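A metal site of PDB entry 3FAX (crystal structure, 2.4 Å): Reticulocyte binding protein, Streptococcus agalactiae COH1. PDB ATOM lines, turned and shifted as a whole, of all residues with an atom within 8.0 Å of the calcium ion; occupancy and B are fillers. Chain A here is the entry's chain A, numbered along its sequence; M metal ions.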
ATOM      1  N   ARG A 265      27.398  -2.882  -8.068  1.00  0.00           N
ATOM      2  CA  ARG A 265      26.448  -4.014  -8.102  1.00  0.00           C
ATOM      3  C   ARG A 265      25.004  -3.589  -8.405  1.00  0.00           C
ATOM      4  O   ARG A 265      24.270  -4.315  -9.058  1.00  0.00           O
ATOM      5  CB  ARG A 265      26.514  -4.854  -6.814  1.00  0.00           C
ATOM      6  CG  ARG A 265      26.750  -4.090  -5.517  1.00  0.00           C
ATOM      7  CD  ARG A 265      27.079  -5.024  -4.360  1.00  0.00           C
ATOM      8  NE  ARG A 265      26.790  -4.380  -3.089  1.00  0.00           N
ATOM      9  CZ  ARG A 265      26.665  -4.996  -1.922  1.00  0.00           C
ATOM     10  NH1 ARG A 265      26.813  -6.320  -1.815  1.00  0.00           N
ATOM     11  NH2 ARG A 265      26.372  -4.287  -0.840  1.00  0.00           N
ATOM     12  N   GLN A 504      21.603 -14.879   4.076  1.00  0.00           N
ATOM     13  CA  GLN A 504      20.844 -13.644   4.097  1.00  0.00           C
ATOM     14  C   GLN A 504      21.118 -12.760   5.328  1.00  0.00           C
ATOM     15  O   GLN A 504      21.182 -11.550   5.204  1.00  0.00           O
ATOM     16  CB  GLN A 504      19.355 -13.939   3.951  1.00  0.00           C
ATOM     17  CG  GLN A 504      18.936 -14.244   2.504  1.00  0.00           C
ATOM     18  CD  GLN A 504      17.489 -14.727   2.370  1.00  0.00           C
ATOM     19  OE1 GLN A 504      16.827 -15.053   3.365  1.00  0.00           O
ATOM     20  NE2 GLN A 504      17.006 -14.804   1.127  1.00  0.00           N
ATOM     21  N   TRP A 506      23.798 -12.385   6.921  1.00  0.00           N
ATOM     22  CA  TRP A 506      25.129 -11.801   6.762  1.00  0.00           C
ATOM     23  C   TRP A 506      25.075 -10.410   6.109  1.00  0.00           C
ATOM     24  O   TRP A 506      26.015  -9.630   6.228  1.00  0.00           O
ATOM     25  CB  TRP A 506      25.967 -12.761   5.902  1.00  0.00           C
ATOM     26  CG  TRP A 506      27.381 -12.380   5.629  1.00  0.00           C
ATOM     27  CD1 TRP A 506      28.279 -11.850   6.504  1.00  0.00           C
ATOM     28  CD2 TRP A 506      28.079 -12.552   4.389  1.00  0.00           C
ATOM     29  NE1 TRP A 506      29.492 -11.651   5.883  1.00  0.00           N
ATOM     30  CE2 TRP A 506      29.389 -12.077   4.585  1.00  0.00           C
ATOM     31  CE3 TRP A 506      27.716 -13.048   3.127  1.00  0.00           C
ATOM     32  CZ2 TRP A 506      30.347 -12.093   3.563  1.00  0.00           C
ATOM     33  CZ3 TRP A 506      28.661 -13.049   2.115  1.00  0.00           C
ATOM     34  CH2 TRP A 506      29.965 -12.574   2.340  1.00  0.00           C
ATOM     35  N   MET A 507      23.966 -10.111   5.427  1.00  0.00           N
ATOM     36  CA  MET A 507      23.828  -8.857   4.694  1.00  0.00           C
ATOM     37  C   MET A 507      23.856  -7.604   5.581  1.00  0.00           C
ATOM     38  O   MET A 507      24.206  -6.527   5.094  1.00  0.00           O
ATOM     39  CB  MET A 507      22.561  -8.871   3.847  1.00  0.00           C
ATOM     40  CG  MET A 507      22.536  -9.926   2.753  1.00  0.00           C
ATOM     41  SD  MET A 507      23.915  -9.831   1.586  1.00  0.00           S
ATOM     42  CE  MET A 507      25.047 -11.031   2.279  1.00  0.00           C
ATOM     43  N   LYS A 508      23.474  -7.736   6.850  1.00  0.00           N
ATOM     44  CA  LYS A 508      23.612  -6.646   7.852  1.00  0.00           C
ATOM     45  C   LYS A 508      25.052  -6.157   7.921  1.00  0.00           C
ATOM     46  O   LYS A 508      25.311  -4.948   7.989  1.00  0.00           O
ATOM     47  CB  LYS A 508      23.278  -7.125   9.262  1.00  0.00           C
ATOM     48  CG  LYS A 508      21.887  -7.604   9.530  1.00  0.00           C
ATOM     49  CD  LYS A 508      21.806  -8.192  10.937  1.00  0.00           C
ATOM     50  CE  LYS A 508      20.639  -9.165  11.088  1.00  0.00           C
ATOM     51  NZ  LYS A 508      19.302  -8.526  10.934  1.00  0.00           N
ATOM     52  N   SER A 509      25.979  -7.106   7.937  1.00  0.00           N
ATOM     53  CA  SER A 509      27.372  -6.865   8.280  1.00  0.00           C
ATOM     54  C   SER A 509      28.360  -7.153   7.148  1.00  0.00           C
ATOM     55  O   SER A 509      29.444  -7.688   7.384  1.00  0.00           O
ATOM     56  CB  SER A 509      27.734  -7.676   9.538  1.00  0.00           C
ATOM     57  OG  SER A 509      27.262  -9.018   9.456  1.00  0.00           O
ATOM     58  N   THR A 510      27.969  -6.825   5.911  1.00  0.00           N
ATOM     59  CA  THR A 510      28.903  -6.658   4.780  1.00  0.00           C
ATOM     60  C   THR A 510      28.209  -5.903   3.651  1.00  0.00           C
ATOM     61  O   THR A 510      26.984  -5.863   3.589  1.00  0.00           O
ATOM     62  CB  THR A 510      29.435  -7.998   4.188  1.00  0.00           C
ATOM     63  OG1 THR A 510      28.452  -9.036   4.332  1.00  0.00           O
ATOM     64  CG2 THR A 510      30.743  -8.410   4.846  1.00  0.00           C
ATOM     65  N   ASP A 511      28.997  -5.303   2.773  1.00  0.00           N
ATOM     66  CA  ASP A 511      28.476  -4.742   1.542  1.00  0.00           C
ATOM     67  C   ASP A 511      29.323  -5.258   0.389  1.00  0.00           C
ATOM     68  O   ASP A 511      29.731  -4.502  -0.499  1.00  0.00           O
ATOM     69  CB  ASP A 511      28.447  -3.206   1.591  1.00  0.00           C
ATOM     70  CG  ASP A 511      27.335  -2.666   2.473  1.00  0.00           C
ATOM     71  OD1 ASP A 511      26.216  -3.222   2.454  1.00  0.00           O
ATOM     72  OD2 ASP A 511      27.592  -1.674   3.192  1.00  0.00           O
ATOM     73  N   THR A 512      29.556  -6.555   0.410  1.00  0.00           N
ATOM     74  CA  THR A 512      30.415  -7.219  -0.547  1.00  0.00           C
ATOM     75  C   THR A 512      29.586  -8.055  -1.518  1.00  0.00           C
ATOM     76  O   THR A 512      29.518  -7.753  -2.705  1.00  0.00           O
ATOM     77  CB  THR A 512      31.396  -8.152   0.181  1.00  0.00           C
ATOM     78  OG1 THR A 512      30.673  -9.108   0.969  1.00  0.00           O
ATOM     79  CG2 THR A 512      32.334  -7.333   1.093  1.00  0.00           C
ATOM     80  N   VAL A 513      28.967  -9.104  -0.984  1.00  0.00           N
ATOM     81  CA  VAL A 513      28.269 -10.100  -1.790  1.00  0.00           C
ATOM     82  C   VAL A 513      26.771  -9.934  -1.606  1.00  0.00           C
ATOM     83  O   VAL A 513      26.288  -9.862  -0.481  1.00  0.00           O
ATOM     84  CB  VAL A 513      28.653 -11.515  -1.344  1.00  0.00           C
ATOM     85  CG1 VAL A 513      27.845 -12.565  -2.111  1.00  0.00           C
ATOM     86  CG2 VAL A 513      30.160 -11.747  -1.519  1.00  0.00           C
ATOM     87  N   PHE A 558      14.830 -10.701   5.661  1.00  0.00           N
ATOM     88  CA  PHE A 558      16.181 -10.414   6.151  1.00  0.00           C
ATOM     89  C   PHE A 558      16.475  -8.918   6.018  1.00  0.00           C
ATOM     90  O   PHE A 558      15.751  -8.210   5.314  1.00  0.00           O
ATOM     91  CB  PHE A 558      17.256 -11.248   5.411  1.00  0.00           C
ATOM     92  CG  PHE A 558      17.561 -10.777   4.007  1.00  0.00           C
ATOM     93  CD1 PHE A 558      18.555  -9.833   3.773  1.00  0.00           C
ATOM     94  CD2 PHE A 558      16.884 -11.312   2.919  1.00  0.00           C
ATOM     95  CE1 PHE A 558      18.844  -9.404   2.492  1.00  0.00           C
ATOM     96  CE2 PHE A 558      17.177 -10.890   1.615  1.00  0.00           C
ATOM     97  CZ  PHE A 558      18.158  -9.934   1.405  1.00  0.00           C
ATOM     98  N   GLU A 559      17.509  -8.446   6.703  1.00  0.00           N
ATOM     99  CA  GLU A 559      17.831  -7.025   6.728  1.00  0.00           C
ATOM    100  C   GLU A 559      18.826  -6.665   5.629  1.00  0.00           C
ATOM    101  O   GLU A 559      19.989  -7.091   5.658  1.00  0.00           O
ATOM    102  CB  GLU A 559      18.377  -6.588   8.107  1.00  0.00           C
ATOM    103  CG  GLU A 559      18.174  -5.083   8.367  1.00  0.00           C
ATOM    104  CD  GLU A 559      19.028  -4.541   9.498  1.00  0.00           C
ATOM    105  OE1 GLU A 559      19.043  -5.141  10.596  1.00  0.00           O
ATOM    106  OE2 GLU A 559      19.689  -3.494   9.300  1.00  0.00           O
ATOM    107  N   ALA A 560      18.370  -5.874   4.661  1.00  0.00           N
ATOM    108  CA  ALA A 560      19.225  -5.348   3.600  1.00  0.00           C
ATOM    109  C   ALA A 560      19.471  -3.869   3.884  1.00  0.00           C
ATOM    110  O   ALA A 560      18.604  -3.043   3.605  1.00  0.00           O
ATOM    111  CB  ALA A 560      18.576  -5.529   2.238  1.00  0.00           C
ATOM    112  N   ASP A 561      20.642  -3.547   4.448  1.00  0.00           N
ATOM    113  CA  ASP A 561      20.987  -2.145   4.763  1.00  0.00           C
ATOM    114  C   ASP A 561      21.628  -1.413   3.578  1.00  0.00           C
ATOM    115  O   ASP A 561      22.031  -0.253   3.701  1.00  0.00           O
ATOM    116  CB  ASP A 561      21.854  -2.043   6.021  1.00  0.00           C
ATOM    117  CG  ASP A 561      23.208  -2.731   5.876  1.00  0.00           C
ATOM    118  OD1 ASP A 561      23.417  -3.469   4.894  1.00  0.00           O
ATOM    119  OD2 ASP A 561      24.063  -2.530   6.764  1.00  0.00           O
ATOM    120  N   SER A 562      21.716  -2.095   2.446  1.00  0.00           N
ATOM    121  CA  SER A 562      22.158  -1.482   1.206  1.00  0.00           C
ATOM    122  C   SER A 562      21.442  -2.156   0.029  1.00  0.00           C
ATOM    123  O   SER A 562      21.284  -3.371   0.028  1.00  0.00           O
ATOM    124  CB  SER A 562      23.667  -1.603   1.066  1.00  0.00           C
ATOM    125  OG  SER A 562      24.108  -1.005  -0.127  1.00  0.00           O
ATOM    126  N   PRO A 563      21.010  -1.375  -0.971  1.00  0.00           N
ATOM    127  CA  PRO A 563      20.312  -1.991  -2.102  1.00  0.00           C
ATOM    128  C   PRO A 563      21.149  -3.084  -2.757  1.00  0.00           C
ATOM    129  O   PRO A 563      20.594  -4.099  -3.191  1.00  0.00           O
ATOM    130  CB  PRO A 563      20.073  -0.824  -3.062  1.00  0.00           C
ATOM    131  CG  PRO A 563      21.013   0.247  -2.643  1.00  0.00           C
ATOM    132  CD  PRO A 563      21.165   0.083  -1.162  1.00  0.00           C
ATOM    133  N   GLY A 564      22.457  -2.897  -2.808  1.00  0.00           N
ATOM    134  CA  GLY A 564      23.374  -3.887  -3.361  1.00  0.00           C
ATOM    135  C   GLY A 564      23.390  -5.248  -2.693  1.00  0.00           C
ATOM    136  O   GLY A 564      23.939  -6.201  -3.243  1.00  0.00           O
ATOM    137  N   ASP A 565      22.802  -5.348  -1.502  1.00  0.00           N
ATOM    138  CA  ASP A 565      22.670  -6.643  -0.821  1.00  0.00           C
ATOM    139  C   ASP A 565      21.629  -7.548  -1.463  1.00  0.00           C
ATOM    140  O   ASP A 565      21.599  -8.744  -1.187  1.00  0.00           O
ATOM    141  CB  ASP A 565      22.258  -6.448   0.640  1.00  0.00           C
ATOM    142  CG  ASP A 565      23.296  -5.710   1.445  1.00  0.00           C
ATOM    143  OD1 ASP A 565      24.493  -5.760   1.082  1.00  0.00           O
ATOM    144  OD2 ASP A 565      22.908  -5.099   2.456  1.00  0.00           O
ATOM    145  N   VAL A 566      20.762  -6.982  -2.302  1.00  0.00           N
ATOM    146  CA  VAL A 566      19.584  -7.707  -2.788  1.00  0.00           C
ATOM    147  C   VAL A 566      19.676  -7.956  -4.279  1.00  0.00           C
ATOM    148  O   VAL A 566      19.810  -7.031  -5.086  1.00  0.00           O
ATOM    149  CB  VAL A 566      18.278  -6.940  -2.423  1.00  0.00           C
ATOM    150  CG1 VAL A 566      17.052  -7.586  -3.058  1.00  0.00           C
ATOM    151  CG2 VAL A 566      18.126  -6.875  -0.906  1.00  0.00           C
HETATM  152 CA    CA M   1      24.965  -4.771   3.726  1.00  0.00          CA
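The calcium ion is bound by O of Thr 510 (2.3 Å), OD1 of Asp 561 (2.3 Å), O of Met 507 (2.4 Å), OD1 of Asp 511 (2.4 Å), OD2 of Asp 565 (2.4 Å) and OD1 of Asp 565 (2.9 Å).
Five residues have an atom within 4 Å of the calcium ion: Met 507, Thr 510, Asp 511, Asp 561 and Asp 565.
The guanidinium group (NH2) of Arg 265 sits close to the side-chain carboxylate (OD1) of Asp 565 (3.1 Å).
The backbone carbonyl oxygen (O) of Asp 511 sits close to the guanidinium group (NH2) of Arg 265, at 3.4 Å.
The side-chain carboxylate of Asp 565 sits close to the backbone NH of Ser 562 (3.2 Å).
The side-chain hydroxyl of Thr 510 is in hydrogen-bond range of the backbone carbonyl oxygen of Trp 506 (3.1 Å).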
